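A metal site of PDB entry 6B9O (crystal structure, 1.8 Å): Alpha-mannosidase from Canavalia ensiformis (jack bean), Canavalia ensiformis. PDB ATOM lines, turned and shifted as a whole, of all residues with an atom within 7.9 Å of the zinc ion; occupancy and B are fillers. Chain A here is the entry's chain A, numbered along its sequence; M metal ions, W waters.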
ATOM      1  N   HIS A  23      -1.553  -7.327 -27.905  1.00  0.00           N
ATOM      2  CA  HIS A  23      -1.942  -8.702 -28.142  1.00  0.00           C
ATOM      3  C   HIS A  23      -3.050  -9.081 -27.159  1.00  0.00           C
ATOM      4  O   HIS A  23      -2.804  -9.256 -25.971  1.00  0.00           O
ATOM      5  CB  HIS A  23      -0.764  -9.664 -27.982  1.00  0.00           C
ATOM      6  CG  HIS A  23      -1.138 -11.089 -28.238  1.00  0.00           C
ATOM      7  ND1 HIS A  23      -1.693 -11.496 -29.426  1.00  0.00           N
ATOM      8  CD2 HIS A  23      -1.110 -12.180 -27.430  1.00  0.00           C
ATOM      9  CE1 HIS A  23      -1.950 -12.794 -29.371  1.00  0.00           C
ATOM     10  NE2 HIS A  23      -1.626 -13.227 -28.154  1.00  0.00           N
ATOM     11  N   ASP A  24      -4.268  -9.213 -27.660  1.00  0.00           N
ATOM     12  CA  ASP A  24      -5.451  -9.345 -26.820  1.00  0.00           C
ATOM     13  C   ASP A  24      -6.011 -10.745 -27.046  1.00  0.00           C
ATOM     14  O   ASP A  24      -6.747 -10.983 -28.015  1.00  0.00           O
ATOM     15  CB  ASP A  24      -6.467  -8.249 -27.141  1.00  0.00           C
ATOM     16  CG  ASP A  24      -5.880  -6.851 -26.976  1.00  0.00           C
ATOM     17  OD1 ASP A  24      -4.976  -6.668 -26.124  1.00  0.00           O
ATOM     18  OD2 ASP A  24      -6.294  -5.944 -27.728  1.00  0.00           O
ATOM     19  N   ASP A  25      -5.686 -11.671 -26.153  1.00  0.00           N
ATOM     20  CA  ASP A  25      -6.190 -13.028 -26.256  1.00  0.00           C
ATOM     21  C   ASP A  25      -7.691 -13.073 -26.024  1.00  0.00           C
ATOM     22  O   ASP A  25      -8.198 -12.548 -25.028  1.00  0.00           O
ATOM     23  CB  ASP A  25      -5.501 -13.931 -25.241  1.00  0.00           C
ATOM     24  CG  ASP A  25      -4.053 -14.204 -25.612  1.00  0.00           C
ATOM     25  OD1 ASP A  25      -3.809 -14.704 -26.722  1.00  0.00           O
ATOM     26  OD2 ASP A  25      -3.180 -13.915 -24.770  1.00  0.00           O
ATOM     27  N   VAL A  26      -8.419 -13.720 -26.937  1.00  0.00           N
ATOM     28  CA  VAL A  26      -9.847 -13.868 -26.773  1.00  0.00           C
ATOM     29  C   VAL A  26     -10.113 -14.960 -25.742  1.00  0.00           C
ATOM     30  O   VAL A  26     -10.539 -16.075 -26.086  1.00  0.00           O
ATOM     31  CB  VAL A  26     -10.522 -14.128 -28.137  1.00  0.00           C
ATOM     32  CG1 VAL A  26     -12.030 -14.264 -27.977  1.00  0.00           C
ATOM     33  CG2 VAL A  26     -10.229 -12.975 -29.083  1.00  0.00           C
ATOM     34  N   GLY A  27      -9.878 -14.650 -24.467  1.00  0.00           N
ATOM     35  CA  GLY A  27      -9.874 -15.645 -23.415  1.00  0.00           C
ATOM     36  C   GLY A  27      -8.528 -16.334 -23.299  1.00  0.00           C
ATOM     37  O   GLY A  27      -7.876 -16.590 -24.319  1.00  0.00           O
ATOM     38  N   TRP A  28      -8.088 -16.611 -22.082  1.00  0.00           N
ATOM     39  CA  TRP A  28      -6.871 -17.387 -21.799  1.00  0.00           C
ATOM     40  C   TRP A  28      -6.786 -17.616 -20.296  1.00  0.00           C
ATOM     41  O   TRP A  28      -7.242 -18.646 -19.791  1.00  0.00           O
ATOM     42  CB  TRP A  28      -5.595 -16.698 -22.322  1.00  0.00           C
ATOM     43  CG  TRP A  28      -4.367 -17.529 -22.068  1.00  0.00           C
ATOM     44  CD1 TRP A  28      -4.260 -18.905 -22.138  1.00  0.00           C
ATOM     45  CD2 TRP A  28      -3.066 -17.049 -21.693  1.00  0.00           C
ATOM     46  NE1 TRP A  28      -2.977 -19.293 -21.825  1.00  0.00           N
ATOM     47  CE2 TRP A  28      -2.230 -18.173 -21.548  1.00  0.00           C
ATOM     48  CE3 TRP A  28      -2.532 -15.774 -21.437  1.00  0.00           C
ATOM     49  CZ2 TRP A  28      -0.876 -18.072 -21.185  1.00  0.00           C
ATOM     50  CZ3 TRP A  28      -1.190 -15.661 -21.075  1.00  0.00           C
ATOM     51  CH2 TRP A  28      -0.376 -16.816 -20.957  1.00  0.00           C
ATOM     52  N   GLU A  71      -8.522  -8.298 -33.152  1.00  0.00           N
ATOM     53  CA  GLU A  71      -9.523  -9.282 -32.748  1.00  0.00           C
ATOM     54  C   GLU A  71     -10.898  -8.642 -32.693  1.00  0.00           C
ATOM     55  O   GLU A  71     -11.213  -7.863 -31.784  1.00  0.00           O
ATOM     56  CB  GLU A  71      -9.134  -9.900 -31.405  1.00  0.00           C
ATOM     57  CG  GLU A  71      -7.821 -10.740 -31.446  1.00  0.00           C
ATOM     58  CD  GLU A  71      -6.528  -9.918 -31.323  1.00  0.00           C
ATOM     59  OE1 GLU A  71      -6.588  -8.734 -30.954  1.00  0.00           O
ATOM     60  OE2 GLU A  71      -5.435 -10.486 -31.581  1.00  0.00           O
ATOM     61  N   MET A 108      -7.677 -14.411 -33.338  1.00  0.00           N
ATOM     62  CA  MET A 108      -6.433 -14.889 -33.951  1.00  0.00           C
ATOM     63  C   MET A 108      -6.403 -16.397 -33.697  1.00  0.00           C
ATOM     64  O   MET A 108      -6.147 -16.837 -32.581  1.00  0.00           O
ATOM     65  CB  MET A 108      -5.226 -14.175 -33.333  1.00  0.00           C
ATOM     66  CG  MET A 108      -3.876 -14.638 -33.906  1.00  0.00           C
ATOM     67  SD  MET A 108      -2.479 -13.919 -32.995  1.00  0.00           S
ATOM     68  CE  MET A 108      -2.838 -12.172 -33.251  1.00  0.00           C
ATOM     69  N   ILE A 144       0.784 -13.497 -34.416  1.00  0.00           N
ATOM     70  CA  ILE A 144       2.036 -13.241 -33.711  1.00  0.00           C
ATOM     71  C   ILE A 144       2.274 -14.276 -32.610  1.00  0.00           C
ATOM     72  O   ILE A 144       3.425 -14.540 -32.262  1.00  0.00           O
ATOM     73  CB  ILE A 144       2.083 -11.796 -33.160  1.00  0.00           C
ATOM     74  CG1 ILE A 144       0.940 -11.495 -32.197  1.00  0.00           C
ATOM     75  CG2 ILE A 144       2.045 -10.782 -34.306  1.00  0.00           C
ATOM     76  CD1 ILE A 144       1.057 -10.068 -31.567  1.00  0.00           C
ATOM     77  N   ASP A 145       1.213 -14.873 -32.067  1.00  0.00           N
ATOM     78  CA  ASP A 145       1.359 -15.786 -30.916  1.00  0.00           C
ATOM     79  C   ASP A 145       1.120 -17.284 -31.196  1.00  0.00           C
ATOM     80  O   ASP A 145       1.627 -18.103 -30.426  1.00  0.00           O
ATOM     81  CB  ASP A 145       0.419 -15.326 -29.788  1.00  0.00           C
ATOM     82  CG  ASP A 145       0.829 -15.859 -28.394  1.00  0.00           C
ATOM     83  OD1 ASP A 145       1.991 -16.240 -28.199  1.00  0.00           O
ATOM     84  OD2 ASP A 145      -0.040 -15.867 -27.483  1.00  0.00           O
ATOM     85  N   PRO A 146       0.352 -17.698 -32.201  1.00  0.00           N
ATOM     86  CA  PRO A 146       0.080 -19.141 -32.358  1.00  0.00           C
ATOM     87  C   PRO A 146       1.327 -20.029 -32.449  1.00  0.00           C
ATOM     88  O   PRO A 146       2.390 -19.615 -32.906  1.00  0.00           O
ATOM     89  CB  PRO A 146      -0.736 -19.204 -33.652  1.00  0.00           C
ATOM     90  CG  PRO A 146      -1.573 -17.922 -33.525  1.00  0.00           C
ATOM     91  CD  PRO A 146      -0.587 -16.869 -33.071  1.00  0.00           C
ATOM     92  N   PHE A 147       1.152 -21.282 -31.997  1.00  0.00           N
ATOM     93  CA  PHE A 147       2.280 -22.109 -31.575  1.00  0.00           C
ATOM     94  C   PHE A 147       2.718 -23.017 -32.730  1.00  0.00           C
ATOM     95  O   PHE A 147       2.488 -24.215 -32.752  1.00  0.00           O
ATOM     96  CB  PHE A 147       1.906 -22.933 -30.328  1.00  0.00           C
ATOM     97  CG  PHE A 147       0.963 -22.225 -29.376  1.00  0.00           C
ATOM     98  CD1 PHE A 147       1.162 -20.892 -28.983  1.00  0.00           C
ATOM     99  CD2 PHE A 147      -0.115 -22.916 -28.807  1.00  0.00           C
ATOM    100  CE1 PHE A 147       0.288 -20.272 -28.079  1.00  0.00           C
ATOM    101  CE2 PHE A 147      -1.006 -22.298 -27.919  1.00  0.00           C
ATOM    102  CZ  PHE A 147      -0.808 -20.967 -27.550  1.00  0.00           C
ATOM    103  N   ARG A 170       6.569 -17.053 -33.387  1.00  0.00           N
ATOM    104  CA  ARG A 170       6.970 -18.386 -32.959  1.00  0.00           C
ATOM    105  C   ARG A 170       7.344 -19.261 -34.152  1.00  0.00           C
ATOM    106  O   ARG A 170       6.497 -19.557 -35.010  1.00  0.00           O
ATOM    107  CB  ARG A 170       5.846 -19.051 -32.153  1.00  0.00           C
ATOM    108  CG  ARG A 170       5.547 -18.322 -30.857  1.00  0.00           C
ATOM    109  CD  ARG A 170       4.522 -19.081 -30.009  1.00  0.00           C
ATOM    110  NE  ARG A 170       4.059 -18.262 -28.893  1.00  0.00           N
ATOM    111  CZ  ARG A 170       4.775 -18.035 -27.801  1.00  0.00           C
ATOM    112  NH1 ARG A 170       5.975 -18.606 -27.658  1.00  0.00           N
ATOM    113  NH2 ARG A 170       4.297 -17.263 -26.841  1.00  0.00           N
ATOM    114  N   TYR A 210       7.105 -10.950 -29.897  1.00  0.00           N
ATOM    115  CA  TYR A 210       6.322  -9.873 -30.481  1.00  0.00           C
ATOM    116  C   TYR A 210       6.263  -8.641 -29.580  1.00  0.00           C
ATOM    117  O   TYR A 210       5.356  -7.805 -29.734  1.00  0.00           O
ATOM    118  CB  TYR A 210       4.922 -10.382 -30.858  1.00  0.00           C
ATOM    119  CG  TYR A 210       4.170 -11.061 -29.748  1.00  0.00           C
ATOM    120  CD1 TYR A 210       3.523 -10.336 -28.775  1.00  0.00           C
ATOM    121  CD2 TYR A 210       4.067 -12.453 -29.700  1.00  0.00           C
ATOM    122  CE1 TYR A 210       2.804 -10.973 -27.758  1.00  0.00           C
ATOM    123  CE2 TYR A 210       3.338 -13.101 -28.706  1.00  0.00           C
ATOM    124  CZ  TYR A 210       2.733 -12.360 -27.736  1.00  0.00           C
ATOM    125  OH  TYR A 210       2.034 -13.019 -26.725  1.00  0.00           O
ATOM    126  N   ASP A 268       1.231  -8.480 -24.615  1.00  0.00           N
ATOM    127  CA  ASP A 268      -0.072  -8.935 -24.133  1.00  0.00           C
ATOM    128  C   ASP A 268      -0.814  -7.845 -23.384  1.00  0.00           C
ATOM    129  O   ASP A 268      -0.332  -7.342 -22.370  1.00  0.00           O
ATOM    130  CB  ASP A 268       0.113 -10.156 -23.207  1.00  0.00           C
ATOM    131  CG  ASP A 268       0.550 -11.398 -23.960  1.00  0.00           C
ATOM    132  OD1 ASP A 268       0.931 -11.260 -25.130  1.00  0.00           O
ATOM    133  OD2 ASP A 268       0.491 -12.496 -23.388  1.00  0.00           O
ATOM    134  N   PHE A 269      -1.999  -7.463 -23.891  1.00  0.00           N
ATOM    135  CA  PHE A 269      -2.924  -6.564 -23.198  1.00  0.00           C
ATOM    136  C   PHE A 269      -2.262  -5.241 -22.803  1.00  0.00           C
ATOM    137  O   PHE A 269      -2.682  -4.573 -21.845  1.00  0.00           O
ATOM    138  CB  PHE A 269      -3.553  -7.264 -21.989  1.00  0.00           C
ATOM    139  CG  PHE A 269      -4.468  -8.389 -22.390  1.00  0.00           C
ATOM    140  CD1 PHE A 269      -5.724  -8.109 -22.942  1.00  0.00           C
ATOM    141  CD2 PHE A 269      -4.082  -9.706 -22.257  1.00  0.00           C
ATOM    142  CE1 PHE A 269      -6.587  -9.145 -23.342  1.00  0.00           C
ATOM    143  CE2 PHE A 269      -4.950 -10.746 -22.644  1.00  0.00           C
ATOM    144  CZ  PHE A 269      -6.204 -10.450 -23.214  1.00  0.00           C
ATOM    145  N   HIS A 385      -9.955 -19.347 -31.052  1.00  0.00           N
ATOM    146  CA  HIS A 385      -8.808 -18.606 -30.512  1.00  0.00           C
ATOM    147  C   HIS A 385      -7.668 -19.552 -30.148  1.00  0.00           C
ATOM    148  O   HIS A 385      -7.894 -20.717 -29.800  1.00  0.00           O
ATOM    149  CB  HIS A 385      -9.249 -17.791 -29.278  1.00  0.00           C
ATOM    150  CG  HIS A 385      -8.112 -17.327 -28.425  1.00  0.00           C
ATOM    151  ND1 HIS A 385      -7.150 -16.453 -28.896  1.00  0.00           N
ATOM    152  CD2 HIS A 385      -7.767 -17.634 -27.152  1.00  0.00           C
ATOM    153  CE1 HIS A 385      -6.267 -16.229 -27.944  1.00  0.00           C
ATOM    154  NE2 HIS A 385      -6.607 -16.937 -26.876  1.00  0.00           N
ATOM    155  N   HIS A 386      -6.427 -19.052 -30.236  1.00  0.00           N
ATOM    156  CA  HIS A 386      -5.281 -19.952 -30.117  1.00  0.00           C
ATOM    157  C   HIS A 386      -5.040 -20.468 -28.706  1.00  0.00           C
ATOM    158  O   HIS A 386      -4.113 -21.285 -28.554  1.00  0.00           O
ATOM    159  CB  HIS A 386      -4.011 -19.279 -30.679  1.00  0.00           C
ATOM    160  CG  HIS A 386      -3.713 -17.945 -30.094  1.00  0.00           C
ATOM    161  ND1 HIS A 386      -4.213 -16.772 -30.605  1.00  0.00           N
ATOM    162  CD2 HIS A 386      -2.930 -17.585 -29.036  1.00  0.00           C
ATOM    163  CE1 HIS A 386      -3.777 -15.753 -29.890  1.00  0.00           C
ATOM    164  NE2 HIS A 386      -2.989 -16.226 -28.936  1.00  0.00           N
ATOM    165  N   ASP A 387      -5.846 -20.079 -27.698  1.00  0.00           N
ATOM    166  CA  ASP A 387      -5.907 -20.822 -26.434  1.00  0.00           C
ATOM    167  C   ASP A 387      -7.230 -21.558 -26.232  1.00  0.00           C
ATOM    168  O   ASP A 387      -7.423 -22.144 -25.169  1.00  0.00           O
ATOM    169  CB  ASP A 387      -5.672 -19.884 -25.229  1.00  0.00           C
ATOM    170  CG  ASP A 387      -4.359 -19.150 -25.309  1.00  0.00           C
ATOM    171  OD1 ASP A 387      -3.309 -19.831 -25.191  1.00  0.00           O
ATOM    172  OD2 ASP A 387      -4.365 -17.899 -25.485  1.00  0.00           O
ATOM    173  N   TYR A 625       0.539 -27.418 -23.095  1.00  0.00           N
ATOM    174  CA  TYR A 625       1.171 -27.090 -24.373  1.00  0.00           C
ATOM    175  C   TYR A 625       2.144 -28.169 -24.834  1.00  0.00           C
ATOM    176  O   TYR A 625       2.100 -28.602 -25.992  1.00  0.00           O
ATOM    177  CB  TYR A 625       1.992 -25.794 -24.281  1.00  0.00           C
ATOM    178  CG  TYR A 625       1.277 -24.538 -23.842  1.00  0.00           C
ATOM    179  CD1 TYR A 625       1.060 -24.267 -22.500  1.00  0.00           C
ATOM    180  CD2 TYR A 625       0.879 -23.588 -24.773  1.00  0.00           C
ATOM    181  CE1 TYR A 625       0.439 -23.091 -22.081  1.00  0.00           C
ATOM    182  CE2 TYR A 625       0.262 -22.408 -24.367  1.00  0.00           C
ATOM    183  CZ  TYR A 625       0.039 -22.182 -23.018  1.00  0.00           C
ATOM    184  OH  TYR A 625      -0.556 -21.013 -22.590  1.00  0.00           O
HETATM  185 ZN    ZN M   1      -2.044 -15.108 -27.491  1.00  0.00          ZN
HETATM  186  O   HOH W   1      -2.035 -16.697 -25.832  1.00  0.00           O
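O of Met 108 sits at hydrogen-bond distance from ND1 of His 386 (2.8 Å).
NH2 of Arg 170 is in salt-bridge range of OD1 of Asp 145.
A ring nitrogen (ND1) of His 385 sits close to a ring nitrogen (ND1) of His 386 (3.4 Å).
O of His 23 lies within hydrogen-bond range of N of Phe 269, at 2.9 Å.
Within 4 Å of the zinc ion: His 23, Asp 25, Asp 145 and His 386.
The nearest printed residue that does not touch the zinc ion is Asp 387 (4.1 Å).
The side-chain carboxylate (OD1) of Asp 25 is bound to the zinc ion, 2.0 Å away.
A ring nitrogen (NE2) of His 23 binds the zinc ion (2.0 Å).
The zinc ion is bound by a ring nitrogen (NE2) of His 386, 2.1 Å away.
OD2 of Asp 145 is bound to the zinc ion, at 2.1 Å.
The zinc ion is bound by water W1, at 2.3 Å.
Water W1 bridges OD2 of Asp 387 (2.6 Å) and OD2 of Asp 25 (3.2 Å).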
